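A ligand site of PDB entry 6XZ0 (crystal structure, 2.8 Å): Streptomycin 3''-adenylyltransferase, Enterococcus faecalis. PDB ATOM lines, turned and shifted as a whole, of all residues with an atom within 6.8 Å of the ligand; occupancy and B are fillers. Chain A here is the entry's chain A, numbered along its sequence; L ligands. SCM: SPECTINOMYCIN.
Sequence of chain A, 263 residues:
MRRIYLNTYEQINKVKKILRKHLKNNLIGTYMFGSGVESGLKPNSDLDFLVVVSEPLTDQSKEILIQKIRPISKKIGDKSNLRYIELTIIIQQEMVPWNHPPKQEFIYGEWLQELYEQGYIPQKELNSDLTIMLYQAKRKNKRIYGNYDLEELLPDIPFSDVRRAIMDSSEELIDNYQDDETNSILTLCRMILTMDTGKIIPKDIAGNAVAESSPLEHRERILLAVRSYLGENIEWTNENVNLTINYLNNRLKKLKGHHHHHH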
ATOM      1  N   ASP A  46      18.405  16.583 -23.888  1.00  0.00           N
ATOM      2  CA  ASP A  46      18.340  17.353 -22.660  1.00  0.00           C
ATOM      3  C   ASP A  46      19.468  16.943 -21.720  1.00  0.00           C
ATOM      4  O   ASP A  46      20.004  15.825 -21.801  1.00  0.00           O
ATOM      5  CB  ASP A  46      16.990  17.170 -21.970  1.00  0.00           C
ATOM      6  CG  ASP A  46      15.836  17.688 -22.800  1.00  0.00           C
ATOM      7  OD1 ASP A  46      16.086  18.416 -23.786  1.00  0.00           O
ATOM      8  OD2 ASP A  46      14.672  17.373 -22.477  1.00  0.00           O
ATOM      9  N   ASP A  48      20.479  15.923 -18.266  1.00  0.00           N
ATOM     10  CA  ASP A  48      19.982  15.345 -17.015  1.00  0.00           C
ATOM     11  C   ASP A  48      21.160  15.137 -16.074  1.00  0.00           C
ATOM     12  O   ASP A  48      21.975  14.234 -16.277  1.00  0.00           O
ATOM     13  CB  ASP A  48      19.253  14.035 -17.289  1.00  0.00           C
ATOM     14  CG  ASP A  48      18.327  14.113 -18.488  1.00  0.00           C
ATOM     15  OD1 ASP A  48      17.529  15.072 -18.564  1.00  0.00           O
ATOM     16  OD2 ASP A  48      18.401  13.216 -19.353  1.00  0.00           O
ATOM     17  N   LYS A  74      17.292  26.385 -20.540  1.00  0.00           N
ATOM     18  CA  LYS A  74      16.396  26.757 -21.617  1.00  0.00           C
ATOM     19  C   LYS A  74      14.954  26.786 -21.122  1.00  0.00           C
ATOM     20  O   LYS A  74      14.492  25.840 -20.480  1.00  0.00           O
ATOM     21  CB  LYS A  74      16.510  25.781 -22.782  1.00  0.00           C
ATOM     22  CG  LYS A  74      15.400  25.921 -23.821  1.00  0.00           C
ATOM     23  CD  LYS A  74      15.022  24.590 -24.443  1.00  0.00           C
ATOM     24  CE  LYS A  74      13.944  24.765 -25.506  1.00  0.00           C
ATOM     25  NZ  LYS A  74      13.723  23.525 -26.313  1.00  0.00           N
ATOM     26  N   ILE A  76      10.806  26.803 -21.786  1.00  0.00           N
ATOM     27  CA  ILE A  76      10.014  25.903 -22.633  1.00  0.00           C
ATOM     28  C   ILE A  76       9.697  26.540 -23.975  1.00  0.00           C
ATOM     29  O   ILE A  76       9.630  25.847 -24.998  1.00  0.00           O
ATOM     30  CB  ILE A  76       8.744  25.470 -21.886  1.00  0.00           C
ATOM     31  CG1 ILE A  76       9.074  25.087 -20.450  1.00  0.00           C
ATOM     32  CG2 ILE A  76       8.067  24.312 -22.615  1.00  0.00           C
ATOM     33  CD1 ILE A  76       7.858  24.792 -19.596  1.00  0.00           C
ATOM     34  N   TYR A  84      17.116  22.072 -22.167  1.00  0.00           N
ATOM     35  CA  TYR A  84      16.610  22.011 -20.804  1.00  0.00           C
ATOM     36  C   TYR A  84      17.659  21.414 -19.877  1.00  0.00           C
ATOM     37  O   TYR A  84      18.447  20.540 -20.260  1.00  0.00           O
ATOM     38  CB  TYR A  84      15.337  21.174 -20.729  1.00  0.00           C
ATOM     39  CG  TYR A  84      14.182  21.704 -21.541  1.00  0.00           C
ATOM     40  CD1 TYR A  84      13.674  22.973 -21.319  1.00  0.00           C
ATOM     41  CD2 TYR A  84      13.596  20.931 -22.532  1.00  0.00           C
ATOM     42  CE1 TYR A  84      12.610  23.464 -22.057  1.00  0.00           C
ATOM     43  CE2 TYR A  84      12.540  21.408 -23.277  1.00  0.00           C
ATOM     44  CZ  TYR A  84      12.051  22.667 -23.042  1.00  0.00           C
ATOM     45  OH  TYR A  84      10.995  23.144 -23.787  1.00  0.00           O
ATOM     46  N   ILE A  85      17.665  21.895 -18.641  1.00  0.00           N
ATOM     47  CA  ILE A  85      18.534  21.377 -17.588  1.00  0.00           C
ATOM     48  C   ILE A  85      17.654  20.790 -16.504  1.00  0.00           C
ATOM     49  O   ILE A  85      16.836  21.500 -15.897  1.00  0.00           O
ATOM     50  CB  ILE A  85      19.476  22.455 -17.036  1.00  0.00           C
ATOM     51  CG1 ILE A  85      20.615  22.707 -18.015  1.00  0.00           C
ATOM     52  CG2 ILE A  85      20.010  22.045 -15.669  1.00  0.00           C
ATOM     53  CD1 ILE A  85      21.609  23.732 -17.551  1.00  0.00           C
ATOM     54  N   GLU A  86      17.809  19.492 -16.266  1.00  0.00           N
ATOM     55  CA  GLU A  86      17.036  18.743 -15.273  1.00  0.00           C
ATOM     56  C   GLU A  86      18.034  18.123 -14.293  1.00  0.00           C
ATOM     57  O   GLU A  86      18.766  17.201 -14.655  1.00  0.00           O
ATOM     58  CB  GLU A  86      16.173  17.677 -15.946  1.00  0.00           C
ATOM     59  CG  GLU A  86      14.864  17.377 -15.243  1.00  0.00           C
ATOM     60  CD  GLU A  86      13.996  16.427 -16.042  1.00  0.00           C
ATOM     61  OE1 GLU A  86      13.635  16.761 -17.181  1.00  0.00           O
ATOM     62  OE2 GLU A  86      13.681  15.326 -15.522  1.00  0.00           O
ATOM     63  N   GLY A 109      13.617  21.704 -12.569  1.00  0.00           N
ATOM     64  CA  GLY A 109      12.938  21.373 -13.797  1.00  0.00           C
ATOM     65  C   GLY A 109      12.189  22.569 -14.317  1.00  0.00           C
ATOM     66  O   GLY A 109      11.599  23.323 -13.528  1.00  0.00           O
ATOM     67  N   GLU A 110      12.194  22.782 -15.642  1.00  0.00           N
ATOM     68  CA  GLU A 110      11.578  23.986 -16.175  1.00  0.00           C
ATOM     69  C   GLU A 110      10.064  23.897 -16.239  1.00  0.00           C
ATOM     70  O   GLU A 110       9.403  24.932 -16.381  1.00  0.00           O
ATOM     71  CB  GLU A 110      12.158  24.300 -17.556  1.00  0.00           C
ATOM     72  CG  GLU A 110      12.450  25.776 -17.754  1.00  0.00           C
ATOM     73  CD  GLU A 110      13.787  26.182 -17.158  1.00  0.00           C
ATOM     74  OE1 GLU A 110      14.817  25.947 -17.808  1.00  0.00           O
ATOM     75  OE2 GLU A 110      13.800  26.721 -16.028  1.00  0.00           O
ATOM     76  N   TRP A 111       9.487  22.705 -16.110  1.00  0.00           N
ATOM     77  CA  TRP A 111       8.046  22.608 -15.920  1.00  0.00           C
ATOM     78  C   TRP A 111       7.619  23.117 -14.551  1.00  0.00           C
ATOM     79  O   TRP A 111       6.429  23.352 -14.335  1.00  0.00           O
ATOM     80  CB  TRP A 111       7.577  21.156 -16.110  1.00  0.00           C
ATOM     81  CG  TRP A 111       7.949  20.234 -14.982  1.00  0.00           C
ATOM     82  CD1 TRP A 111       7.171  19.905 -13.907  1.00  0.00           C
ATOM     83  CD2 TRP A 111       9.178  19.508 -14.835  1.00  0.00           C
ATOM     84  NE1 TRP A 111       7.841  19.025 -13.098  1.00  0.00           N
ATOM     85  CE2 TRP A 111       9.076  18.770 -13.642  1.00  0.00           C
ATOM     86  CE3 TRP A 111      10.350  19.421 -15.580  1.00  0.00           C
ATOM     87  CZ2 TRP A 111      10.106  17.947 -13.185  1.00  0.00           C
ATOM     88  CZ3 TRP A 111      11.365  18.600 -15.131  1.00  0.00           C
ATOM     89  CH2 TRP A 111      11.240  17.877 -13.938  1.00  0.00           C
ATOM     90  N   LEU A 112       8.567  23.293 -13.628  1.00  0.00           N
ATOM     91  CA  LEU A 112       8.303  23.818 -12.298  1.00  0.00           C
ATOM     92  C   LEU A 112       8.642  25.288 -12.168  1.00  0.00           C
ATOM     93  O   LEU A 112       8.699  25.804 -11.042  1.00  0.00           O
ATOM     94  CB  LEU A 112       9.081  23.007 -11.255  1.00  0.00           C
ATOM     95  CG  LEU A 112       8.656  21.545 -11.141  1.00  0.00           C
ATOM     96  CD1 LEU A 112       9.550  20.791 -10.178  1.00  0.00           C
ATOM     97  CD2 LEU A 112       7.208  21.472 -10.711  1.00  0.00           C
ATOM     98  N   ASN A 127       9.729  10.365  -4.574  1.00  0.00           N
ATOM     99  CA  ASN A 127       9.491  10.309  -6.005  1.00  0.00           C
ATOM    100  C   ASN A 127       9.750   8.897  -6.499  1.00  0.00           C
ATOM    101  O   ASN A 127      10.864   8.369  -6.352  1.00  0.00           O
ATOM    102  CB  ASN A 127      10.381  11.310  -6.751  1.00  0.00           C
ATOM    103  CG  ASN A 127      10.069  11.396  -8.230  1.00  0.00           C
ATOM    104  OD1 ASN A 127       9.114  10.790  -8.714  1.00  0.00           O
ATOM    105  ND2 ASN A 127      10.870  12.160  -8.965  1.00  0.00           N
ATOM    106  N   ASP A 129       9.453   8.027  -9.711  1.00  0.00           N
ATOM    107  CA  ASP A 129      10.188   8.131 -10.968  1.00  0.00           C
ATOM    108  C   ASP A 129      11.695   8.023 -10.739  1.00  0.00           C
ATOM    109  O   ASP A 129      12.422   7.537 -11.615  1.00  0.00           O
ATOM    110  CB  ASP A 129       9.861   9.458 -11.662  1.00  0.00           C
ATOM    111  CG  ASP A 129       8.659   9.360 -12.581  1.00  0.00           C
ATOM    112  OD1 ASP A 129       8.332   8.231 -13.004  1.00  0.00           O
ATOM    113  OD2 ASP A 129       8.063  10.410 -12.885  1.00  0.00           O
ATOM    114  N   MET A 133      15.345   6.276 -12.677  1.00  0.00           N
ATOM    115  CA  MET A 133      16.452   7.174 -12.968  1.00  0.00           C
ATOM    116  C   MET A 133      17.759   6.620 -12.426  1.00  0.00           C
ATOM    117  O   MET A 133      18.753   6.507 -13.157  1.00  0.00           O
ATOM    118  CB  MET A 133      16.173   8.559 -12.390  1.00  0.00           C
ATOM    119  CG  MET A 133      14.801   9.124 -12.751  1.00  0.00           C
ATOM    120  SD  MET A 133      14.725  10.927 -12.674  1.00  0.00           S
ATOM    121  CE  MET A 133      16.019  11.277 -11.493  1.00  0.00           C
ATOM    122  N   LEU A 173       0.345   8.491 -14.619  1.00  0.00           N
ATOM    123  CA  LEU A 173       0.470   9.198 -15.889  1.00  0.00           C
ATOM    124  C   LEU A 173      -0.838   9.188 -16.675  1.00  0.00           C
ATOM    125  O   LEU A 173      -1.116  10.139 -17.399  1.00  0.00           O
ATOM    126  CB  LEU A 173       1.586   8.545 -16.720  1.00  0.00           C
ATOM    127  CG  LEU A 173       1.939   9.132 -18.074  1.00  0.00           C
ATOM    128  CD1 LEU A 173       2.077  10.644 -17.967  1.00  0.00           C
ATOM    129  CD2 LEU A 173       3.215   8.491 -18.602  1.00  0.00           C
ATOM    130  N   ASP A 179      -2.091  18.037 -21.576  1.00  0.00           N
ATOM    131  CA  ASP A 179      -1.171  19.141 -21.831  1.00  0.00           C
ATOM    132  C   ASP A 179       0.288  18.704 -21.908  1.00  0.00           C
ATOM    133  O   ASP A 179       1.155  19.505 -22.246  1.00  0.00           O
ATOM    134  CB  ASP A 179      -1.343  20.243 -20.784  1.00  0.00           C
ATOM    135  CG  ASP A 179      -2.560  21.112 -21.048  1.00  0.00           C
ATOM    136  OD1 ASP A 179      -3.339  21.354 -20.100  1.00  0.00           O
ATOM    137  OD2 ASP A 179      -2.733  21.550 -22.207  1.00  0.00           O
ATOM    138  N   ASP A 180       0.571  17.436 -21.595  1.00  0.00           N
ATOM    139  CA  ASP A 180       1.874  16.868 -21.907  1.00  0.00           C
ATOM    140  C   ASP A 180       1.700  15.645 -22.790  1.00  0.00           C
ATOM    141  O   ASP A 180       2.269  14.578 -22.529  1.00  0.00           O
ATOM    142  CB  ASP A 180       2.646  16.509 -20.629  1.00  0.00           C
ATOM    143  CG  ASP A 180       4.139  16.374 -20.885  1.00  0.00           C
ATOM    144  OD1 ASP A 180       4.613  16.874 -21.923  1.00  0.00           O
ATOM    145  OD2 ASP A 180       4.837  15.781 -20.035  1.00  0.00           O
ATOM    146  N   THR A 182       2.568  14.951 -25.992  1.00  0.00           N
ATOM    147  CA  THR A 182       3.670  14.470 -26.829  1.00  0.00           C
ATOM    148  C   THR A 182       4.677  13.664 -26.024  1.00  0.00           C
ATOM    149  O   THR A 182       5.215  12.663 -26.510  1.00  0.00           O
ATOM    150  CB  THR A 182       4.359  15.656 -27.524  1.00  0.00           C
ATOM    151  OG1 THR A 182       5.611  15.222 -28.057  1.00  0.00           O
ATOM    152  CG2 THR A 182       4.582  16.791 -26.539  1.00  0.00           C
ATOM    153  N   ASN A 183       4.945  14.067 -24.781  1.00  0.00           N
ATOM    154  CA  ASN A 183       5.978  13.403 -23.993  1.00  0.00           C
ATOM    155  C   ASN A 183       5.454  12.158 -23.296  1.00  0.00           C
ATOM    156  O   ASN A 183       6.181  11.158 -23.182  1.00  0.00           O
ATOM    157  CB  ASN A 183       6.549  14.373 -22.954  1.00  0.00           C
ATOM    158  CG  ASN A 183       7.702  13.775 -22.182  1.00  0.00           C
ATOM    159  OD1 ASN A 183       7.601  13.526 -20.977  1.00  0.00           O
ATOM    160  ND2 ASN A 183       8.806  13.509 -22.864  1.00  0.00           N
ATOM    161  N   SER A 184       4.199  12.186 -22.839  1.00  0.00           N
ATOM    162  CA  SER A 184       3.665  11.058 -22.082  1.00  0.00           C
ATOM    163  C   SER A 184       3.358   9.864 -22.974  1.00  0.00           C
ATOM    164  O   SER A 184       3.401   8.712 -22.519  1.00  0.00           O
ATOM    165  CB  SER A 184       2.416  11.481 -21.313  1.00  0.00           C
ATOM    166  OG  SER A 184       1.676  12.464 -22.027  1.00  0.00           O
ATOM    167  N   THR A 187       6.835   8.248 -23.406  1.00  0.00           N
ATOM    168  CA  THR A 187       7.348   7.698 -22.149  1.00  0.00           C
ATOM    169  C   THR A 187       6.769   6.317 -21.866  1.00  0.00           C
ATOM    170  O   THR A 187       7.492   5.413 -21.432  1.00  0.00           O
ATOM    171  CB  THR A 187       7.040   8.651 -20.995  1.00  0.00           C
ATOM    172  OG1 THR A 187       7.682   9.911 -21.230  1.00  0.00           O
ATOM    173  CG2 THR A 187       7.530   8.070 -19.678  1.00  0.00           C
ATOM    174  N   LYS A 203      13.187   8.110 -25.968  1.00  0.00           N
ATOM    175  CA  LYS A 203      11.802   8.204 -26.381  1.00  0.00           C
ATOM    176  C   LYS A 203      11.656   8.438 -27.878  1.00  0.00           C
ATOM    177  O   LYS A 203      10.583   8.177 -28.427  1.00  0.00           O
ATOM    178  CB  LYS A 203      11.108   9.326 -25.597  1.00  0.00           C
ATOM    179  CG  LYS A 203      11.230   9.157 -24.103  1.00  0.00           C
ATOM    180  CD  LYS A 203      11.945  10.319 -23.463  1.00  0.00           C
ATOM    181  CE  LYS A 203      11.185  11.599 -23.676  1.00  0.00           C
ATOM    182  NZ  LYS A 203      11.807  12.752 -22.939  1.00  0.00           N
ATOM    183  N   TYR A 229       8.387  16.045 -30.646  1.00  0.00           N
ATOM    184  CA  TYR A 229       9.583  16.194 -29.835  1.00  0.00           C
ATOM    185  C   TYR A 229      10.782  16.659 -30.661  1.00  0.00           C
ATOM    186  O   TYR A 229      11.762  17.151 -30.097  1.00  0.00           O
ATOM    187  CB  TYR A 229       9.923  14.887 -29.138  1.00  0.00           C
ATOM    188  CG  TYR A 229      10.557  15.077 -27.790  1.00  0.00           C
ATOM    189  CD1 TYR A 229      10.783  14.000 -26.957  1.00  0.00           C
ATOM    190  CD2 TYR A 229      10.926  16.336 -27.337  1.00  0.00           C
ATOM    191  CE1 TYR A 229      11.366  14.173 -25.731  1.00  0.00           C
ATOM    192  CE2 TYR A 229      11.513  16.515 -26.104  1.00  0.00           C
ATOM    193  CZ  TYR A 229      11.724  15.427 -25.296  1.00  0.00           C
ATOM    194  OH  TYR A 229      12.313  15.571 -24.059  1.00  0.00           O
HETATM  195  O1  SCM L   1      10.331  18.340 -19.582  1.00  0.00           O
HETATM  196  C2  SCM L   1      10.264  19.627 -20.215  1.00  0.00           C
HETATM  197  C2M SCM L   1      11.323  20.486 -19.583  1.00  0.00           C
HETATM  198  C3  SCM L   1       8.860  20.176 -20.051  1.00  0.00           C
HETATM  199  C4  SCM L   1       7.847  19.184 -20.566  1.00  0.00           C
HETATM  200  O4  SCM L   1       6.945  19.510 -21.305  1.00  0.00           O
HETATM  201  C5  SCM L   1       8.066  17.736 -20.085  1.00  0.00           C
HETATM  202  O5  SCM L   1       7.336  16.856 -20.868  1.00  0.00           O
HETATM  203  C6  SCM L   1       9.548  17.358 -20.202  1.00  0.00           C
HETATM  204  O1B SCM L   1       7.575  17.685 -18.755  1.00  0.00           O
HETATM  205  O2B SCM L   1       9.805  16.155 -19.510  1.00  0.00           O
HETATM  206  C7  SCM L   1       7.922  16.463 -18.069  1.00  0.00           C
HETATM  207  C8  SCM L   1       7.461  16.578 -16.614  1.00  0.00           C
HETATM  208  N8  SCM L   1       5.998  16.623 -16.519  1.00  0.00           N
HETATM  209  C8M SCM L   1       5.456  17.979 -16.392  1.00  0.00           C
HETATM  210  C9  SCM L   1       7.940  15.382 -15.806  1.00  0.00           C
HETATM  211  O9  SCM L   1       7.263  14.210 -16.246  1.00  0.00           O
HETATM  212  C10 SCM L   1       9.453  15.207 -15.912  1.00  0.00           C
HETATM  213  N10 SCM L   1       9.863  14.089 -15.045  1.00  0.00           N
HETATM  214  C1M SCM L   1       9.934  12.794 -15.736  1.00  0.00           C
HETATM  215  C11 SCM L   1       9.883  15.045 -17.378  1.00  0.00           C
HETATM  216  O11 SCM L   1      11.301  14.943 -17.451  1.00  0.00           O
HETATM  217  C12 SCM L   1       9.427  16.277 -18.130  1.00  0.00           C
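Tyr 84 touches the ligand. Trp 111 touches the ligand. Hydrophobic or aromatic side chains that line the ligand: Tyr 84 and Trp 111. Of the 23 residues printed, 5 come within 4 Å of the ligand. The nearest printed residue that does not touch the ligand is Asp 129 (4.2 Å).
OD2 of Asp 180 lies within salt-bridge range of N8 of the ligand (3.8 Å). The side-chain amide oxygen of Asn 183 lies close to an oxygen (O5) of the ligand (3.3 Å). The side-chain carboxylate (OE1) of Glu 86 is in hydrogen-bond range of an oxygen (O11) of the ligand, 3.0 Å away.
NZ of Lys 203 lies close to ND2 of Asn 183 (3.1 Å). O of Asn 183 lies within hydrogen-bond range of OG1 of Thr 187. OH of Tyr 84 sits close to O of Ile 76.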
